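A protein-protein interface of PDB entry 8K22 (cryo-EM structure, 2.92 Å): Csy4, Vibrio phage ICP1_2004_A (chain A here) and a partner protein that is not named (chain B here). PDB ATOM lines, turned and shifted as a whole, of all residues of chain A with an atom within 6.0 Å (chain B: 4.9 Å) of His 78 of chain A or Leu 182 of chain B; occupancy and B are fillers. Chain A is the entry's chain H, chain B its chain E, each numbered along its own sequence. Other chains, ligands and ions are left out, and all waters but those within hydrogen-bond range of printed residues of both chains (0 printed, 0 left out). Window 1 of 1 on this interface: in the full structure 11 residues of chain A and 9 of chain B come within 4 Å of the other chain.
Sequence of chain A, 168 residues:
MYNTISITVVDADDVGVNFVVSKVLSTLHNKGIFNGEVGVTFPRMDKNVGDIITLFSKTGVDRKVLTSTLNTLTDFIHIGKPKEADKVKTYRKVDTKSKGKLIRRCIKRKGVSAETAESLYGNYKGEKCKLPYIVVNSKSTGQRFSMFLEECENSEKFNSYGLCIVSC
The side-chain carboxylate of Glu 185 of chain B lies within hydrogen-bond range of the side-chain hydroxyl of Ser 6 of chain A, 2.6 Å away.
The guanidinium group (NH1) of Arg 144 of chain B is in hydrogen-bond range of the backbone carbonyl oxygen (O) of Ile 77 of chain A.
NE2 of His 78 of chain A lies close to OE1 of Glu 179 of chain B, 3.3 Å away.
The side-chain carboxylate (OE2) of Glu 183 of chain B lies within salt-bridge range of the side-chain amino group (NZ) of Lys 81 of chain A (3.3 Å).
N of Val 10 of chain A is in hydrogen-bond range of O of Phe 76 of chain A, 3.3 Å away.
OE2 of Glu 179 of chain B is in salt-bridge range of NE of Arg 144 of chain B (2.9 Å).
N of Gly 80 of chain A is in hydrogen-bond range of O of Ser 6 of chain A (3.2 Å).
The backbone NH (N) of Thr 8 of chain A lies within hydrogen-bond range of the backbone carbonyl oxygen (O) of His 78 of chain A, at 2.8 Å.
CD2 of Leu 182 of chain B touches CG2 of Thr 8 of chain A (3.7 Å).
Glu 185 of chain B touches Thr 8 of chain A (OE2 to OG1, 3.6 Å).
Arg 144 of chain B touches Val 10 of chain A (NH1 to CG2, 3.4 Å).
Val 10 of chain A touches Leu 182 of chain B (CG1 to CD1, 3.4 Å).
CD2 of His 78 of chain A touches CD of Arg 144 of chain B, 3.9 Å away.
O of Leu 182 of chain B touches CE1 of His 78 of chain A (3.1 Å).
Glu 183 of chain B touches His 78 of chain A (N to CE1, 3.7 Å).
CA of Gly 80 of chain A touches OE2 of Glu 183 of chain B, 3.5 Å away.
Printed residues of chain B within 4 Å of Ser 6 of chain A: Glu 185.
His 78 of chain A touches just these residues of chain B: Arg 144 (3.9 Å), Glu 179 (3.1 Å), Leu 182 (3.1 Å) and Glu 183 (3.7 Å).
Of the printed residues of chain A, Glu 179 of chain B touches His 78 (3.1 Å).
Leu 182 of chain B touches just these residues of chain A: Thr 8 (3.7 Å), Val 10 (3.4 Å) and His 78 (3.1 Å).
The nearest printed residue of chain B that does not touch His 78 of chain A is Tyr 184 of chain B (6.1 Å).
The nearest printed residue of chain A that does not touch Leu 182 of chain B is Ser 6 of chain A (5.3 Å).
Along chain B the printed residues that touch a printed residue of chain A span positions 144 to 185.
Among the printed residues, Asp or Glu carboxylates within 4 Å of a Lys or Arg side-chain nitrogen of the other chain: Lys 81 of chain A with Glu 183 of chain B.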
ATOM      1  N   SER A   6      11.528  12.234 -16.993  1.00  0.00           N
ATOM      2  CA  SER A   6      10.957  11.385 -18.025  1.00  0.00           C
ATOM      3  C   SER A   6      10.929   9.934 -17.573  1.00  0.00           C
ATOM      4  O   SER A   6      11.887   9.443 -16.970  1.00  0.00           O
ATOM      5  CB  SER A   6      11.762  11.499 -19.315  1.00  0.00           C
ATOM      6  OG  SER A   6      10.943  11.274 -20.439  1.00  0.00           O
ATOM      7  N   ILE A   7       9.826   9.254 -17.871  1.00  0.00           N
ATOM      8  CA  ILE A   7       9.651   7.829 -17.626  1.00  0.00           C
ATOM      9  C   ILE A   7       9.150   7.227 -18.931  1.00  0.00           C
ATOM     10  O   ILE A   7       7.964   7.341 -19.257  1.00  0.00           O
ATOM     11  CB  ILE A   7       8.662   7.560 -16.479  1.00  0.00           C
ATOM     12  CG1 ILE A   7       9.187   8.115 -15.158  1.00  0.00           C
ATOM     13  CG2 ILE A   7       8.426   6.080 -16.298  1.00  0.00           C
ATOM     14  CD1 ILE A   7       8.120   8.234 -14.100  1.00  0.00           C
ATOM     15  N   THR A   8      10.049   6.624 -19.696  1.00  0.00           N
ATOM     16  CA  THR A   8       9.729   6.114 -21.018  1.00  0.00           C
ATOM     17  C   THR A   8       9.610   4.602 -20.958  1.00  0.00           C
ATOM     18  O   THR A   8      10.520   3.921 -20.475  1.00  0.00           O
ATOM     19  CB  THR A   8      10.799   6.512 -22.034  1.00  0.00           C
ATOM     20  OG1 THR A   8      10.973   7.934 -22.017  1.00  0.00           O
ATOM     21  CG2 THR A   8      10.396   6.073 -23.429  1.00  0.00           C
ATOM     22  N   VAL A   9       8.491   4.099 -21.480  1.00  0.00           N
ATOM     23  CA  VAL A   9       8.259   2.670 -21.522  1.00  0.00           C
ATOM     24  C   VAL A   9       9.001   2.053 -22.663  1.00  0.00           C
ATOM     25  O   VAL A   9       8.826   2.451 -23.805  1.00  0.00           O
ATOM     26  CB  VAL A   9       6.783   2.381 -21.676  1.00  0.00           C
ATOM     27  CG1 VAL A   9       6.559   0.907 -21.912  1.00  0.00           C
ATOM     28  CG2 VAL A   9       6.045   2.838 -20.436  1.00  0.00           C
ATOM     29  N   VAL A  10       9.858   1.091 -22.353  1.00  0.00           N
ATOM     30  CA  VAL A  10      10.665   0.453 -23.362  1.00  0.00           C
ATOM     31  C   VAL A  10      10.260  -0.981 -23.426  1.00  0.00           C
ATOM     32  O   VAL A  10       9.443  -1.388 -22.624  1.00  0.00           O
ATOM     33  CB  VAL A  10      12.149   0.554 -22.974  1.00  0.00           C
ATOM     34  CG1 VAL A  10      12.338   1.742 -22.079  1.00  0.00           C
ATOM     35  CG2 VAL A  10      12.640  -0.644 -22.178  1.00  0.00           C
ATOM     36  N   PHE A  76      11.273  -3.074 -18.061  1.00  0.00           N
ATOM     37  CA  PHE A  76      10.887  -2.404 -19.301  1.00  0.00           C
ATOM     38  C   PHE A  76      10.569  -0.934 -19.046  1.00  0.00           C
ATOM     39  O   PHE A  76       9.537  -0.413 -19.470  1.00  0.00           O
ATOM     40  CB  PHE A  76       9.710  -3.110 -19.976  1.00  0.00           C
ATOM     41  CG  PHE A  76       8.759  -3.763 -19.020  1.00  0.00           C
ATOM     42  CD1 PHE A  76       8.062  -3.017 -18.087  1.00  0.00           C
ATOM     43  CD2 PHE A  76       8.568  -5.131 -19.058  1.00  0.00           C
ATOM     44  CE1 PHE A  76       7.197  -3.623 -17.210  1.00  0.00           C
ATOM     45  CE2 PHE A  76       7.703  -5.741 -18.184  1.00  0.00           C
ATOM     46  CZ  PHE A  76       7.021  -4.986 -17.258  1.00  0.00           C
ATOM     47  N   ILE A  77      11.456  -0.246 -18.332  1.00  0.00           N
ATOM     48  CA  ILE A  77      11.323   1.187 -18.118  1.00  0.00           C
ATOM     49  C   ILE A  77      12.673   1.850 -18.361  1.00  0.00           C
ATOM     50  O   ILE A  77      13.724   1.206 -18.339  1.00  0.00           O
ATOM     51  CB  ILE A  77      10.773   1.514 -16.709  1.00  0.00           C
ATOM     52  CG1 ILE A  77       9.841   2.717 -16.771  1.00  0.00           C
ATOM     53  CG2 ILE A  77      11.885   1.716 -15.680  1.00  0.00           C
ATOM     54  CD1 ILE A  77       8.620   2.473 -17.609  1.00  0.00           C
ATOM     55  N   HIS A  78      12.625   3.149 -18.641  1.00  0.00           N
ATOM     56  CA  HIS A  78      13.822   3.960 -18.770  1.00  0.00           C
ATOM     57  C   HIS A  78      13.544   5.326 -18.168  1.00  0.00           C
ATOM     58  O   HIS A  78      12.493   5.916 -18.418  1.00  0.00           O
ATOM     59  CB  HIS A  78      14.246   4.088 -20.234  1.00  0.00           C
ATOM     60  CG  HIS A  78      15.160   5.239 -20.499  1.00  0.00           C
ATOM     61  ND1 HIS A  78      14.706   6.463 -20.938  1.00  0.00           N
ATOM     62  CD2 HIS A  78      16.500   5.360 -20.367  1.00  0.00           C
ATOM     63  CE1 HIS A  78      15.730   7.284 -21.078  1.00  0.00           C
ATOM     64  NE2 HIS A  78      16.831   6.638 -20.742  1.00  0.00           N
ATOM     65  N   ILE A  79      14.472   5.820 -17.357  1.00  0.00           N
ATOM     66  CA  ILE A  79      14.296   7.096 -16.674  1.00  0.00           C
ATOM     67  C   ILE A  79      15.396   8.036 -17.140  1.00  0.00           C
ATOM     68  O   ILE A  79      16.586   7.730 -16.993  1.00  0.00           O
ATOM     69  CB  ILE A  79      14.325   6.943 -15.145  1.00  0.00           C
ATOM     70  CG1 ILE A  79      13.573   5.686 -14.704  1.00  0.00           C
ATOM     71  CG2 ILE A  79      13.723   8.169 -14.493  1.00  0.00           C
ATOM     72  CD1 ILE A  79      12.082   5.736 -14.937  1.00  0.00           C
ATOM     73  N   GLY A  80      15.001   9.177 -17.697  1.00  0.00           N
ATOM     74  CA  GLY A  80      15.966  10.190 -18.055  1.00  0.00           C
ATOM     75  C   GLY A  80      16.330  11.079 -16.881  1.00  0.00           C
ATOM     76  O   GLY A  80      15.632  11.127 -15.870  1.00  0.00           O
ATOM     77  N   LYS A  81      17.454  11.781 -17.025  1.00  0.00           N
ATOM     78  CA  LYS A  81      17.885  12.711 -15.995  1.00  0.00           C
ATOM     79  C   LYS A  81      16.936  13.907 -15.936  1.00  0.00           C
ATOM     80  O   LYS A  81      16.288  14.237 -16.933  1.00  0.00           O
ATOM     81  CB  LYS A  81      19.324  13.172 -16.249  1.00  0.00           C
ATOM     82  CG  LYS A  81      20.350  12.059 -16.115  1.00  0.00           C
ATOM     83  CD  LYS A  81      21.469  12.167 -17.128  1.00  0.00           C
ATOM     84  CE  LYS A  81      20.966  11.886 -18.523  1.00  0.00           C
ATOM     85  NZ  LYS A  81      20.331  10.546 -18.613  1.00  0.00           N
ATOM     86  N   ARG B 144      20.979   0.021 -17.844  1.00  0.00           N
ATOM     87  CA  ARG B 144      20.627  -0.371 -19.206  1.00  0.00           C
ATOM     88  C   ARG B 144      21.836  -0.306 -20.132  1.00  0.00           C
ATOM     89  O   ARG B 144      22.070  -1.223 -20.932  1.00  0.00           O
ATOM     90  CB  ARG B 144      19.501   0.521 -19.728  1.00  0.00           C
ATOM     91  CG  ARG B 144      18.452   0.864 -18.684  1.00  0.00           C
ATOM     92  CD  ARG B 144      17.294   1.654 -19.276  1.00  0.00           C
ATOM     93  NE  ARG B 144      17.113   1.407 -20.702  1.00  0.00           N
ATOM     94  CZ  ARG B 144      16.287   0.502 -21.206  1.00  0.00           C
ATOM     95  NH1 ARG B 144      15.569  -0.288 -20.424  1.00  0.00           N
ATOM     96  NH2 ARG B 144      16.185   0.380 -22.525  1.00  0.00           N
ATOM     97  N   LYS B 178      19.201   3.632 -29.760  1.00  0.00           N
ATOM     98  CA  LYS B 178      17.899   3.515 -29.120  1.00  0.00           C
ATOM     99  C   LYS B 178      17.954   4.110 -27.718  1.00  0.00           C
ATOM    100  O   LYS B 178      17.006   4.777 -27.297  1.00  0.00           O
ATOM    101  CB  LYS B 178      17.504   2.023 -29.133  1.00  0.00           C
ATOM    102  CG  LYS B 178      16.513   1.371 -28.116  1.00  0.00           C
ATOM    103  CD  LYS B 178      15.225   2.129 -27.771  1.00  0.00           C
ATOM    104  CE  LYS B 178      14.192   1.193 -27.167  1.00  0.00           C
ATOM    105  NZ  LYS B 178      14.804   0.260 -26.181  1.00  0.00           N
ATOM    106  N   GLU B 179      19.064   3.907 -27.006  1.00  0.00           N
ATOM    107  CA  GLU B 179      19.230   4.479 -25.673  1.00  0.00           C
ATOM    108  C   GLU B 179      19.275   6.003 -25.720  1.00  0.00           C
ATOM    109  O   GLU B 179      18.633   6.682 -24.908  1.00  0.00           O
ATOM    110  CB  GLU B 179      20.504   3.928 -25.033  1.00  0.00           C
ATOM    111  CG  GLU B 179      20.569   3.993 -23.511  1.00  0.00           C
ATOM    112  CD  GLU B 179      19.302   3.511 -22.825  1.00  0.00           C
ATOM    113  OE1 GLU B 179      18.406   4.336 -22.550  1.00  0.00           O
ATOM    114  OE2 GLU B 179      19.198   2.294 -22.565  1.00  0.00           O
ATOM    115  N   TYR B 180      20.017   6.557 -26.682  1.00  0.00           N
ATOM    116  CA  TYR B 180      20.068   8.008 -26.818  1.00  0.00           C
ATOM    117  C   TYR B 180      18.757   8.575 -27.352  1.00  0.00           C
ATOM    118  O   TYR B 180      18.438   9.739 -27.088  1.00  0.00           O
ATOM    119  CB  TYR B 180      21.240   8.406 -27.709  1.00  0.00           C
ATOM    120  CG  TYR B 180      22.528   8.565 -26.942  1.00  0.00           C
ATOM    121  CD1 TYR B 180      22.850   9.769 -26.332  1.00  0.00           C
ATOM    122  CD2 TYR B 180      23.413   7.507 -26.811  1.00  0.00           C
ATOM    123  CE1 TYR B 180      24.022   9.916 -25.623  1.00  0.00           C
ATOM    124  CE2 TYR B 180      24.587   7.643 -26.108  1.00  0.00           C
ATOM    125  CZ  TYR B 180      24.886   8.848 -25.517  1.00  0.00           C
ATOM    126  OH  TYR B 180      26.058   8.981 -24.811  1.00  0.00           O
ATOM    127  N   ALA B 181      17.994   7.779 -28.104  1.00  0.00           N
ATOM    128  CA  ALA B 181      16.652   8.195 -28.498  1.00  0.00           C
ATOM    129  C   ALA B 181      15.710   8.205 -27.303  1.00  0.00           C
ATOM    130  O   ALA B 181      14.826   9.064 -27.207  1.00  0.00           O
ATOM    131  CB  ALA B 181      16.118   7.272 -29.589  1.00  0.00           C
ATOM    132  N   LEU B 182      15.877   7.242 -26.394  1.00  0.00           N
ATOM    133  CA  LEU B 182      15.079   7.212 -25.174  1.00  0.00           C
ATOM    134  C   LEU B 182      15.430   8.372 -24.259  1.00  0.00           C
ATOM    135  O   LEU B 182      14.571   8.850 -23.513  1.00  0.00           O
ATOM    136  CB  LEU B 182      15.278   5.889 -24.437  1.00  0.00           C
ATOM    137  CG  LEU B 182      14.603   4.647 -25.022  1.00  0.00           C
ATOM    138  CD1 LEU B 182      14.553   3.538 -23.988  1.00  0.00           C
ATOM    139  CD2 LEU B 182      13.216   4.941 -25.583  1.00  0.00           C
ATOM    140  N   GLU B 183      16.684   8.824 -24.294  1.00  0.00           N
ATOM    141  CA  GLU B 183      17.046  10.051 -23.592  1.00  0.00           C
ATOM    142  C   GLU B 183      16.348  11.275 -24.168  1.00  0.00           C
ATOM    143  O   GLU B 183      15.728  12.051 -23.432  1.00  0.00           O
ATOM    144  CB  GLU B 183      18.560  10.256 -23.624  1.00  0.00           C
ATOM    145  CG  GLU B 183      19.145  11.518 -22.916  1.00  0.00           C
ATOM    146  CD  GLU B 183      18.664  11.895 -21.499  1.00  0.00           C
ATOM    147  OE1 GLU B 183      19.180  12.925 -21.019  1.00  0.00           O
ATOM    148  OE2 GLU B 183      17.903  11.192 -20.806  1.00  0.00           O
ATOM    149  N   TYR B 184      16.438  11.472 -25.481  1.00  0.00           N
ATOM    150  CA  TYR B 184      16.076  12.748 -26.079  1.00  0.00           C
ATOM    151  C   TYR B 184      14.674  12.745 -26.681  1.00  0.00           C
ATOM    152  O   TYR B 184      14.397  13.553 -27.575  1.00  0.00           O
ATOM    153  CB  TYR B 184      17.119  13.148 -27.122  1.00  0.00           C
ATOM    154  CG  TYR B 184      18.429  13.570 -26.496  1.00  0.00           C
ATOM    155  CD1 TYR B 184      18.598  14.849 -25.994  1.00  0.00           C
ATOM    156  CD2 TYR B 184      19.495  12.686 -26.404  1.00  0.00           C
ATOM    157  CE1 TYR B 184      19.794  15.240 -25.418  1.00  0.00           C
ATOM    158  CE2 TYR B 184      20.693  13.065 -25.832  1.00  0.00           C
ATOM    159  CZ  TYR B 184      20.835  14.345 -25.341  1.00  0.00           C
ATOM    160  OH  TYR B 184      22.023  14.733 -24.770  1.00  0.00           O
ATOM    161  N   GLU B 185      13.809  11.835 -26.220  1.00  0.00           N
ATOM    162  CA  GLU B 185      12.350  11.917 -26.369  1.00  0.00           C
ATOM    163  C   GLU B 185      11.892  11.866 -27.823  1.00  0.00           C
ATOM    164  O   GLU B 185      10.912  12.515 -28.193  1.00  0.00           O
ATOM    165  CB  GLU B 185      11.800  13.185 -25.700  1.00  0.00           C
ATOM    166  CG  GLU B 185      12.103  13.368 -24.207  1.00  0.00           C
ATOM    167  CD  GLU B 185      11.261  12.509 -23.272  1.00  0.00           C
ATOM    168  OE1 GLU B 185      10.690  13.084 -22.323  1.00  0.00           O
ATOM    169  OE2 GLU B 185      11.195  11.274 -23.431  1.00  0.00           O
